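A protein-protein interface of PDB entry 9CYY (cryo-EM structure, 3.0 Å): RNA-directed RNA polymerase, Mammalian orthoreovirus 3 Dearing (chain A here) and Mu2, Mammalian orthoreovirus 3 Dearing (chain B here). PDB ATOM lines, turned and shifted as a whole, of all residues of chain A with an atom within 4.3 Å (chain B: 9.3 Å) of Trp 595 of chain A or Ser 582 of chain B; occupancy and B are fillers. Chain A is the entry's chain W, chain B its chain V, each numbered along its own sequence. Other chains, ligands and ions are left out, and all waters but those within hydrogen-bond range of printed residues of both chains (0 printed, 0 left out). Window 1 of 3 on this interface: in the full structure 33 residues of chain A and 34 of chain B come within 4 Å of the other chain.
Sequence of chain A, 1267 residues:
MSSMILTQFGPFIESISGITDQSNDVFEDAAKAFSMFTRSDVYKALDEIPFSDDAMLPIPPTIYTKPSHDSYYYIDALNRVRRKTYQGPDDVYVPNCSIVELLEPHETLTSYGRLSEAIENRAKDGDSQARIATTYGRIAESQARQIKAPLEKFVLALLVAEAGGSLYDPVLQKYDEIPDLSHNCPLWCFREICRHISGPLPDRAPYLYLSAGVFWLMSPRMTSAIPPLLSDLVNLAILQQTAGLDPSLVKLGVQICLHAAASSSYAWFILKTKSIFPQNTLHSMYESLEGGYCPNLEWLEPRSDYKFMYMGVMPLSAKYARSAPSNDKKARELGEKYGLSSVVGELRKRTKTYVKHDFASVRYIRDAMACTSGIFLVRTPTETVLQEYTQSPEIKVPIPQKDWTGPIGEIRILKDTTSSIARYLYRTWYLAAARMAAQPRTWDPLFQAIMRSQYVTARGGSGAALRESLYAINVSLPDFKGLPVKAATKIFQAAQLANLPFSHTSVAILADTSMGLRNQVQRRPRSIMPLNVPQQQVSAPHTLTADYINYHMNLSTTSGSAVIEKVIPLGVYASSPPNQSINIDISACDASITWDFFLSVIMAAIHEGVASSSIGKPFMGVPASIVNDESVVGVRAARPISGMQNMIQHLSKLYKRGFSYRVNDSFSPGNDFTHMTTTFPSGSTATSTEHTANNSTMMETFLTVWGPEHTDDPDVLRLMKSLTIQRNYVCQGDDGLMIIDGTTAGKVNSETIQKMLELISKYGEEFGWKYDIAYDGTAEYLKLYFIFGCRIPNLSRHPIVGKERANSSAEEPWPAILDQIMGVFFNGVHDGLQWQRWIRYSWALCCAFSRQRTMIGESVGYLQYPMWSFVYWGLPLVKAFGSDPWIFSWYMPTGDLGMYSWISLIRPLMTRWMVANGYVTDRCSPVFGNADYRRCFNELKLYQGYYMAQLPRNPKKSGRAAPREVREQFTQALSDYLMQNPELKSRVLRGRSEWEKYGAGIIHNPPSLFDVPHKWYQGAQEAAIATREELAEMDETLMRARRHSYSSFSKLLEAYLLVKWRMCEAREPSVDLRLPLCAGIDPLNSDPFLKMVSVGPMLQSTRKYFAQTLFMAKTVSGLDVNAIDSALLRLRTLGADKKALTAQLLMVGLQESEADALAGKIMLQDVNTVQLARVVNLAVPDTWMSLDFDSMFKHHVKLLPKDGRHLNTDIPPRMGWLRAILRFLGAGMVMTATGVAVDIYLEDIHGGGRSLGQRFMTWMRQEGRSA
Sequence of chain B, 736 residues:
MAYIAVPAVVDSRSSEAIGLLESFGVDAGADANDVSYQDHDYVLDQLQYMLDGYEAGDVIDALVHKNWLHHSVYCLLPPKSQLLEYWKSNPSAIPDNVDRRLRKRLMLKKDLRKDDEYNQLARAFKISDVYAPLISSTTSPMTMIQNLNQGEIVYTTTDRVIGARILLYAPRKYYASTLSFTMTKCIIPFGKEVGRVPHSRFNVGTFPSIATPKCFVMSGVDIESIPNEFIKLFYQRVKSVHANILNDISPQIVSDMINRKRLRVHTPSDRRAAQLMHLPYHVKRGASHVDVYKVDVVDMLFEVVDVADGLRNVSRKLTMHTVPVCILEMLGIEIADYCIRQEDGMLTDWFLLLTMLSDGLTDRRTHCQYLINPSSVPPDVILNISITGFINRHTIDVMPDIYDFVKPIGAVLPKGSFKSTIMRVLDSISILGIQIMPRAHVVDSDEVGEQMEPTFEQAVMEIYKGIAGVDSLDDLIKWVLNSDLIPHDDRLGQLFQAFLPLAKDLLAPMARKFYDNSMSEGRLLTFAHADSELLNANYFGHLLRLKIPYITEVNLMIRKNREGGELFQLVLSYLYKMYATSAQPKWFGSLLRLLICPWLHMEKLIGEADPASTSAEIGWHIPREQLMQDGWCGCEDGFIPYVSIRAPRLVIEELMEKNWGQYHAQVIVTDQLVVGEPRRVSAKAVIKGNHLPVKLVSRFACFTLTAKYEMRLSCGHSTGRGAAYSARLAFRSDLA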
ATOM      1  N   GLN A 401     -11.298 -24.021 -10.017  1.00  0.00           N
ATOM      2  CA  GLN A 401     -10.060 -24.789  -9.937  1.00  0.00           C
ATOM      3  C   GLN A 401      -9.912 -25.488  -8.593  1.00  0.00           C
ATOM      4  O   GLN A 401      -9.223 -26.511  -8.500  1.00  0.00           O
ATOM      5  CB  GLN A 401      -8.863 -23.879 -10.200  1.00  0.00           C
ATOM      6  CG  GLN A 401      -8.857 -23.264 -11.589  1.00  0.00           C
ATOM      7  CD  GLN A 401      -8.352 -24.227 -12.646  1.00  0.00           C
ATOM      8  OE1 GLN A 401      -7.808 -25.284 -12.330  1.00  0.00           O
ATOM      9  NE2 GLN A 401      -8.535 -23.866 -13.910  1.00  0.00           N
ATOM     10  N   TRP A 404     -10.575 -29.981  -7.833  1.00  0.00           N
ATOM     11  CA  TRP A 404      -9.867 -31.155  -8.317  1.00  0.00           C
ATOM     12  C   TRP A 404      -8.751 -31.517  -7.346  1.00  0.00           C
ATOM     13  O   TRP A 404      -8.016 -30.644  -6.876  1.00  0.00           O
ATOM     14  CB  TRP A 404      -9.292 -30.911  -9.714  1.00  0.00           C
ATOM     15  CG  TRP A 404     -10.329 -30.607 -10.752  1.00  0.00           C
ATOM     16  CD1 TRP A 404     -11.002 -29.433 -10.917  1.00  0.00           C
ATOM     17  CD2 TRP A 404     -10.806 -31.490 -11.773  1.00  0.00           C
ATOM     18  NE1 TRP A 404     -11.871 -29.531 -11.976  1.00  0.00           N
ATOM     19  CE2 TRP A 404     -11.770 -30.784 -12.519  1.00  0.00           C
ATOM     20  CE3 TRP A 404     -10.513 -32.810 -12.130  1.00  0.00           C
ATOM     21  CZ2 TRP A 404     -12.442 -31.353 -13.598  1.00  0.00           C
ATOM     22  CZ3 TRP A 404     -11.183 -33.372 -13.202  1.00  0.00           C
ATOM     23  CH2 TRP A 404     -12.135 -32.645 -13.923  1.00  0.00           C
ATOM     24  N   THR A 594     -13.913 -31.440 -25.647  1.00  0.00           N
ATOM     25  CA  THR A 594     -12.521 -31.102 -25.367  1.00  0.00           C
ATOM     26  C   THR A 594     -12.150 -31.546 -23.961  1.00  0.00           C
ATOM     27  O   THR A 594     -13.007 -31.934 -23.162  1.00  0.00           O
ATOM     28  CB  THR A 594     -12.251 -29.599 -25.518  1.00  0.00           C
ATOM     29  OG1 THR A 594     -13.247 -28.858 -24.802  1.00  0.00           O
ATOM     30  CG2 THR A 594     -12.242 -29.183 -26.982  1.00  0.00           C
ATOM     31  N   TRP A 595     -10.847 -31.469 -23.668  1.00  0.00           N
ATOM     32  CA  TRP A 595     -10.338 -31.899 -22.368  1.00  0.00           C
ATOM     33  C   TRP A 595     -10.792 -30.992 -21.234  1.00  0.00           C
ATOM     34  O   TRP A 595     -10.868 -31.438 -20.084  1.00  0.00           O
ATOM     35  CB  TRP A 595      -8.810 -31.970 -22.391  1.00  0.00           C
ATOM     36  CG  TRP A 595      -8.222 -32.304 -21.049  1.00  0.00           C
ATOM     37  CD1 TRP A 595      -7.797 -31.420 -20.100  1.00  0.00           C
ATOM     38  CD2 TRP A 595      -8.029 -33.609 -20.494  1.00  0.00           C
ATOM     39  NE1 TRP A 595      -7.338 -32.093 -18.996  1.00  0.00           N
ATOM     40  CE2 TRP A 595      -7.470 -33.439 -19.212  1.00  0.00           C
ATOM     41  CE3 TRP A 595      -8.267 -34.905 -20.958  1.00  0.00           C
ATOM     42  CZ2 TRP A 595      -7.146 -34.515 -18.390  1.00  0.00           C
ATOM     43  CZ3 TRP A 595      -7.945 -35.973 -20.141  1.00  0.00           C
ATOM     44  CH2 TRP A 595      -7.390 -35.771 -18.873  1.00  0.00           C
ATOM     45  N   ASP A 596     -11.094 -29.727 -21.529  1.00  0.00           N
ATOM     46  CA  ASP A 596     -11.333 -28.758 -20.465  1.00  0.00           C
ATOM     47  C   ASP A 596     -12.468 -29.200 -19.548  1.00  0.00           C
ATOM     48  O   ASP A 596     -12.365 -29.084 -18.321  1.00  0.00           O
ATOM     49  CB  ASP A 596     -11.631 -27.385 -21.065  1.00  0.00           C
ATOM     50  CG  ASP A 596     -12.147 -26.402 -20.037  1.00  0.00           C
ATOM     51  OD1 ASP A 596     -11.319 -25.793 -19.327  1.00  0.00           O
ATOM     52  OD2 ASP A 596     -13.380 -26.236 -19.940  1.00  0.00           O
ATOM     53  N   PHE A 597     -13.558 -29.706 -20.120  1.00  0.00           N
ATOM     54  CA  PHE A 597     -14.699 -30.141 -19.325  1.00  0.00           C
ATOM     55  C   PHE A 597     -14.925 -31.644 -19.461  1.00  0.00           C
ATOM     56  O   PHE A 597     -14.734 -32.425 -18.510  1.00  0.00           O
ATOM     57  CB  PHE A 597     -15.936 -29.371 -19.802  1.00  0.00           C
ATOM     58  CG  PHE A 597     -17.074 -29.344 -18.827  1.00  0.00           C
ATOM     59  CD1 PHE A 597     -17.166 -28.338 -17.881  1.00  0.00           C
ATOM     60  CD2 PHE A 597     -18.074 -30.298 -18.883  1.00  0.00           C
ATOM     61  CE1 PHE A 597     -18.223 -28.299 -16.994  1.00  0.00           C
ATOM     62  CE2 PHE A 597     -19.131 -30.266 -17.996  1.00  0.00           C
ATOM     63  CZ  PHE A 597     -19.207 -29.264 -17.051  1.00  0.00           C
ATOM     64  N   LEU A 599     -13.599 -34.416 -21.531  1.00  0.00           N
ATOM     65  CA  LEU A 599     -12.596 -35.473 -21.484  1.00  0.00           C
ATOM     66  C   LEU A 599     -12.061 -35.650 -20.072  1.00  0.00           C
ATOM     67  O   LEU A 599     -11.936 -36.774 -19.586  1.00  0.00           O
ATOM     68  CB  LEU A 599     -11.457 -35.187 -22.461  1.00  0.00           C
ATOM     69  CG  LEU A 599     -11.671 -35.583 -23.924  1.00  0.00           C
ATOM     70  CD1 LEU A 599     -11.828 -37.085 -24.050  1.00  0.00           C
ATOM     71  CD2 LEU A 599     -12.849 -34.870 -24.541  1.00  0.00           C
ATOM     72  N   SER A 600     -11.813 -34.546 -19.367  1.00  0.00           N
ATOM     73  CA  SER A 600     -11.368 -34.655 -17.983  1.00  0.00           C
ATOM     74  C   SER A 600     -12.376 -35.433 -17.144  1.00  0.00           C
ATOM     75  O   SER A 600     -12.032 -36.453 -16.521  1.00  0.00           O
ATOM     76  CB  SER A 600     -11.136 -33.262 -17.396  1.00  0.00           C
ATOM     77  OG  SER A 600     -12.316 -32.481 -17.460  1.00  0.00           O
ATOM     78  N   MET A 603     -12.934 -39.218 -18.462  1.00  0.00           N
ATOM     79  CA  MET A 603     -11.766 -40.075 -18.286  1.00  0.00           C
ATOM     80  C   MET A 603     -11.550 -40.404 -16.814  1.00  0.00           C
ATOM     81  O   MET A 603     -11.298 -41.564 -16.460  1.00  0.00           O
ATOM     82  CB  MET A 603     -10.523 -39.420 -18.891  1.00  0.00           C
ATOM     83  CG  MET A 603     -10.574 -39.265 -20.408  1.00  0.00           C
ATOM     84  SD  MET A 603     -10.709 -40.796 -21.347  1.00  0.00           S
ATOM     85  CE  MET A 603      -9.095 -41.501 -21.061  1.00  0.00           C
ATOM     86  N   SER A 652      -5.027 -40.788 -21.696  1.00  0.00           N
ATOM     87  CA  SER A 652      -5.292 -39.506 -21.057  1.00  0.00           C
ATOM     88  C   SER A 652      -4.293 -38.431 -21.473  1.00  0.00           C
ATOM     89  O   SER A 652      -4.671 -37.267 -21.645  1.00  0.00           O
ATOM     90  CB  SER A 652      -5.318 -39.690 -19.543  1.00  0.00           C
ATOM     91  OG  SER A 652      -5.527 -38.454 -18.905  1.00  0.00           O
ATOM     92  N   TYR A 655      -5.326 -37.209 -24.837  1.00  0.00           N
ATOM     93  CA  TYR A 655      -6.528 -36.402 -24.692  1.00  0.00           C
ATOM     94  C   TYR A 655      -6.253 -35.050 -24.046  1.00  0.00           C
ATOM     95  O   TYR A 655      -7.012 -34.101 -24.270  1.00  0.00           O
ATOM     96  CB  TYR A 655      -7.572 -37.171 -23.880  1.00  0.00           C
ATOM     97  CG  TYR A 655      -8.372 -38.155 -24.704  1.00  0.00           C
ATOM     98  CD1 TYR A 655      -8.366 -38.091 -26.090  1.00  0.00           C
ATOM     99  CD2 TYR A 655      -9.121 -39.154 -24.097  1.00  0.00           C
ATOM    100  CE1 TYR A 655      -9.091 -38.988 -26.849  1.00  0.00           C
ATOM    101  CE2 TYR A 655      -9.852 -40.052 -24.848  1.00  0.00           C
ATOM    102  CZ  TYR A 655      -9.831 -39.967 -26.224  1.00  0.00           C
ATOM    103  OH  TYR A 655     -10.554 -40.859 -26.982  1.00  0.00           O
ATOM    104  N   LYS A 656      -5.188 -34.941 -23.252  1.00  0.00           N
ATOM    105  CA  LYS A 656      -4.813 -33.688 -22.619  1.00  0.00           C
ATOM    106  C   LYS A 656      -3.927 -32.807 -23.484  1.00  0.00           C
ATOM    107  O   LYS A 656      -4.017 -31.579 -23.375  1.00  0.00           O
ATOM    108  CB  LYS A 656      -4.094 -33.957 -21.288  1.00  0.00           C
ATOM    109  CG  LYS A 656      -3.896 -32.723 -20.428  1.00  0.00           C
ATOM    110  CD  LYS A 656      -2.966 -33.010 -19.267  1.00  0.00           C
ATOM    111  CE  LYS A 656      -3.668 -33.845 -18.212  1.00  0.00           C
ATOM    112  NZ  LYS A 656      -2.833 -34.021 -16.996  1.00  0.00           N
ATOM    113  N   ASP B 531      -2.599 -21.727 -20.366  1.00  0.00           N
ATOM    114  CA  ASP B 531      -2.441 -22.724 -21.420  1.00  0.00           C
ATOM    115  C   ASP B 531      -3.590 -22.656 -22.419  1.00  0.00           C
ATOM    116  O   ASP B 531      -3.471 -23.144 -23.550  1.00  0.00           O
ATOM    117  CB  ASP B 531      -2.326 -24.118 -20.805  1.00  0.00           C
ATOM    118  CG  ASP B 531      -3.483 -24.450 -19.884  1.00  0.00           C
ATOM    119  OD1 ASP B 531      -4.464 -23.678 -19.839  1.00  0.00           O
ATOM    120  OD2 ASP B 531      -3.405 -25.484 -19.190  1.00  0.00           O
ATOM    121  N   SER B 532      -4.709 -22.053 -22.012  1.00  0.00           N
ATOM    122  CA  SER B 532      -5.876 -21.979 -22.884  1.00  0.00           C
ATOM    123  C   SER B 532      -5.596 -21.137 -24.121  1.00  0.00           C
ATOM    124  O   SER B 532      -6.051 -21.473 -25.220  1.00  0.00           O
ATOM    125  CB  SER B 532      -7.068 -21.419 -22.112  1.00  0.00           C
ATOM    126  OG  SER B 532      -6.730 -20.202 -21.475  1.00  0.00           O
ATOM    127  N   LEU B 535      -3.562 -23.197 -26.488  1.00  0.00           N
ATOM    128  CA  LEU B 535      -4.384 -24.241 -27.088  1.00  0.00           C
ATOM    129  C   LEU B 535      -5.304 -23.670 -28.159  1.00  0.00           C
ATOM    130  O   LEU B 535      -5.506 -24.289 -29.211  1.00  0.00           O
ATOM    131  CB  LEU B 535      -5.194 -24.952 -26.004  1.00  0.00           C
ATOM    132  CG  LEU B 535      -4.430 -26.017 -25.216  1.00  0.00           C
ATOM    133  CD1 LEU B 535      -5.333 -26.675 -24.188  1.00  0.00           C
ATOM    134  CD2 LEU B 535      -3.833 -27.053 -26.153  1.00  0.00           C
ATOM    135  N   ARG B 545       3.390 -26.591 -17.915  1.00  0.00           N
ATOM    136  CA  ARG B 545       2.716 -25.787 -16.902  1.00  0.00           C
ATOM    137  C   ARG B 545       3.641 -25.676 -15.697  1.00  0.00           C
ATOM    138  O   ARG B 545       4.052 -26.699 -15.141  1.00  0.00           O
ATOM    139  CB  ARG B 545       1.389 -26.422 -16.488  1.00  0.00           C
ATOM    140  CG  ARG B 545       0.217 -26.199 -17.427  1.00  0.00           C
ATOM    141  CD  ARG B 545       0.350 -27.011 -18.700  1.00  0.00           C
ATOM    142  NE  ARG B 545      -0.881 -27.015 -19.478  1.00  0.00           N
ATOM    143  CZ  ARG B 545      -1.759 -28.008 -19.480  1.00  0.00           C
ATOM    144  NH1 ARG B 545      -1.541 -29.124 -18.806  1.00  0.00           N
ATOM    145  NH2 ARG B 545      -2.877 -27.885 -20.190  1.00  0.00           N
ATOM    146  N   LYS B 577      -6.589 -16.710 -14.407  1.00  0.00           N
ATOM    147  CA  LYS B 577      -6.686 -17.981 -13.699  1.00  0.00           C
ATOM    148  C   LYS B 577      -8.005 -18.682 -14.002  1.00  0.00           C
ATOM    149  O   LYS B 577      -8.049 -19.911 -14.136  1.00  0.00           O
ATOM    150  CB  LYS B 577      -6.498 -17.792 -12.194  1.00  0.00           C
ATOM    151  CG  LYS B 577      -5.116 -17.288 -11.803  1.00  0.00           C
ATOM    152  CD  LYS B 577      -4.960 -17.194 -10.291  1.00  0.00           C
ATOM    153  CE  LYS B 577      -5.779 -16.071  -9.692  1.00  0.00           C
ATOM    154  NZ  LYS B 577      -5.289 -14.744 -10.134  1.00  0.00           N
ATOM    155  N   MET B 578      -9.098 -17.921 -14.115  1.00  0.00           N
ATOM    156  CA  MET B 578     -10.351 -18.541 -14.540  1.00  0.00           C
ATOM    157  C   MET B 578     -10.253 -19.061 -15.970  1.00  0.00           C
ATOM    158  O   MET B 578     -10.760 -20.145 -16.280  1.00  0.00           O
ATOM    159  CB  MET B 578     -11.518 -17.563 -14.420  1.00  0.00           C
ATOM    160  CG  MET B 578     -11.870 -17.163 -13.007  1.00  0.00           C
ATOM    161  SD  MET B 578     -13.301 -16.072 -13.004  1.00  0.00           S
ATOM    162  CE  MET B 578     -12.560 -14.569 -13.617  1.00  0.00           C
ATOM    163  N   TYR B 579      -9.608 -18.296 -16.853  1.00  0.00           N
ATOM    164  CA  TYR B 579      -9.484 -18.702 -18.249  1.00  0.00           C
ATOM    165  C   TYR B 579      -8.679 -19.986 -18.391  1.00  0.00           C
ATOM    166  O   TYR B 579      -8.968 -20.806 -19.270  1.00  0.00           O
ATOM    167  CB  TYR B 579      -8.838 -17.574 -19.056  1.00  0.00           C
ATOM    168  CG  TYR B 579      -8.828 -17.793 -20.552  1.00  0.00           C
ATOM    169  CD1 TYR B 579      -9.838 -18.510 -21.178  1.00  0.00           C
ATOM    170  CD2 TYR B 579      -7.809 -17.276 -21.338  1.00  0.00           C
ATOM    171  CE1 TYR B 579      -9.829 -18.709 -22.544  1.00  0.00           C
ATOM    172  CE2 TYR B 579      -7.792 -17.470 -22.703  1.00  0.00           C
ATOM    173  CZ  TYR B 579      -8.804 -18.186 -23.301  1.00  0.00           C
ATOM    174  OH  TYR B 579      -8.789 -18.380 -24.661  1.00  0.00           O
ATOM    175  N   ALA B 580      -7.671 -20.176 -17.546  1.00  0.00           N
ATOM    176  CA  ALA B 580      -6.860 -21.381 -17.607  1.00  0.00           C
ATOM    177  C   ALA B 580      -7.703 -22.613 -17.283  1.00  0.00           C
ATOM    178  O   ALA B 580      -8.685 -22.551 -16.540  1.00  0.00           O
ATOM    179  CB  ALA B 580      -5.678 -21.285 -16.643  1.00  0.00           C
ATOM    180  N   THR B 581      -7.303 -23.746 -17.856  1.00  0.00           N
ATOM    181  CA  THR B 581      -8.058 -24.980 -17.715  1.00  0.00           C
ATOM    182  C   THR B 581      -7.603 -25.752 -16.478  1.00  0.00           C
ATOM    183  O   THR B 581      -6.792 -25.280 -15.677  1.00  0.00           O
ATOM    184  CB  THR B 581      -7.923 -25.838 -18.972  1.00  0.00           C
ATOM    185  OG1 THR B 581      -8.779 -26.981 -18.864  1.00  0.00           O
ATOM    186  CG2 THR B 581      -6.491 -26.305 -19.145  1.00  0.00           C
ATOM    187  N   SER B 582      -8.137 -26.961 -16.321  1.00  0.00           N
ATOM    188  CA  SER B 582      -7.876 -27.789 -15.145  1.00  0.00           C
ATOM    189  C   SER B 582      -6.727 -28.739 -15.459  1.00  0.00           C
ATOM    190  O   SER B 582      -6.904 -29.738 -16.163  1.00  0.00           O
ATOM    191  CB  SER B 582      -9.130 -28.553 -14.738  1.00  0.00           C
ATOM    192  OG  SER B 582      -9.584 -29.381 -15.795  1.00  0.00           O
ATOM    193  N   ALA B 583      -5.546 -28.431 -14.930  1.00  0.00           N
ATOM    194  CA  ALA B 583      -4.381 -29.284 -15.098  1.00  0.00           C
ATOM    195  C   ALA B 583      -3.367 -28.952 -14.014  1.00  0.00           C
ATOM    196  O   ALA B 583      -3.338 -27.834 -13.494  1.00  0.00           O
ATOM    197  CB  ALA B 583      -3.754 -29.117 -16.486  1.00  0.00           C
ATOM    198  N   GLN B 584      -2.541 -29.935 -13.678  1.00  0.00           N
ATOM    199  CA  GLN B 584      -1.557 -29.765 -12.617  1.00  0.00           C
ATOM    200  C   GLN B 584      -0.343 -29.004 -13.136  1.00  0.00           C
ATOM    201  O   GLN B 584       0.302 -29.463 -14.085  1.00  0.00           O
ATOM    202  CB  GLN B 584      -1.129 -31.121 -12.074  1.00  0.00           C
ATOM    203  CG  GLN B 584      -0.153 -31.049 -10.912  1.00  0.00           C
ATOM    204  CD  GLN B 584      -0.737 -30.349  -9.703  1.00  0.00           C
ATOM    205  OE1 GLN B 584      -1.560 -30.912  -8.983  1.00  0.00           O
ATOM    206  NE2 GLN B 584      -0.311 -29.114  -9.472  1.00  0.00           N
ATOM    207  N   PRO B 585       0.002 -27.852 -12.555  1.00  0.00           N
ATOM    208  CA  PRO B 585       1.248 -27.171 -12.931  1.00  0.00           C
ATOM    209  C   PRO B 585       2.430 -27.789 -12.198  1.00  0.00           C
ATOM    210  O   PRO B 585       2.446 -27.856 -10.968  1.00  0.00           O
ATOM    211  CB  PRO B 585       1.009 -25.720 -12.490  1.00  0.00           C
ATOM    212  CG  PRO B 585      -0.453 -25.637 -12.124  1.00  0.00           C
ATOM    213  CD  PRO B 585      -0.838 -27.009 -11.694  1.00  0.00           C
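The backbone carbonyl oxygen (O) of Thr 581 of chain B lies within hydrogen-bond range of the side-chain amide nitrogen (NE2) of Gln 401 of chain A (2.9 Å). The side-chain amide nitrogen (NE2) of Gln 401 of chain A is in hydrogen-bond range of the backbone carbonyl oxygen (O) of Ala 580 of chain B (2.9 Å). OD1 of Asp 596 of chain A is in hydrogen-bond range of OG1 of Thr 581 of chain B, at 2.8 Å.
OG of Ser 600 of chain A sits at hydrogen-bond distance from O of Trp 595 of chain A. OD1 of Asp 531 of chain B lies close to N of Thr 581 of chain B (3.5 Å).
Among the printed residues, merely in contact across the chains: Gln 401 of chain A with Lys 577 of chain B (3.99 Å), Gln 401 of chain A with Ser 582 of chain B (3.8 Å), Trp 595 of chain A with Ser 582 of chain B (3.7 Å) and Asp 596 of chain A with Ser 582 of chain B (3.8 Å).
Of the printed residues of chain B, Gln 401 of chain A touches Lys 577, Ala 580, Thr 581 and Ser 582. Trp 404 of chain A touches none of the printed residues of chain B. No residue of chain B comes within 4 Å of Thr 594 of chain A. Trp 595 of chain A touches just one residue of chain B: Ser 582. Printed residues of chain B within 4 Å of Asp 596 of chain A: Thr 581 and Ser 582. No residue of chain B comes within 4 Å of Leu 599 of chain A. No residue of chain B comes within 4 Å of Ser 600 of chain A. No residue of chain B comes within 4 Å of Lys 656 of chain A. Asp 531 of chain B touches none of the printed residues of chain A. Printed residues of chain A within 4 Å of Lys 577 of chain B: Gln 401. Printed residues of chain A within 4 Å of Ala 580 of chain B: Gln 401. Of the printed residues of chain A, Thr 581 of chain B touches Gln 401 (2.9 Å) and Asp 596 (2.8 Å). Of the printed residues of chain A, Ser 582 of chain B touches Gln 401, Trp 595 and Asp 596. The nearest residue of chain B that does not touch Trp 595 of chain A is Thr 581 of chain B (4.7 Å). The nearest printed residue of chain A that does not touch Ser 582 of chain B is Trp 404 of chain A (4.01 Å). The nearest printed residue of chain A that does not touch Thr 581 of chain B is Trp 595 of chain A (4.7 Å).
Printed residues of chain B that touch a printed residue of chain A: Lys 577, Ala 580, Thr 581 and Ser 582. Of the 12 printed residues of chain A, 3 touch a printed residue of chain B. Printed residues of chain A that touch a printed residue of chain B: Gln 401, Trp 595 and Asp 596. Hydrophobic or aromatic side chains of chain A within 4 Å of the printed part of chain B: Trp 595. Among the printed residues, 7 pairs touch across the chains. Among the printed residues, no Asp or Glu carboxylate lies within 4 Å of a Lys or Arg side-chain nitrogen of the other chain.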
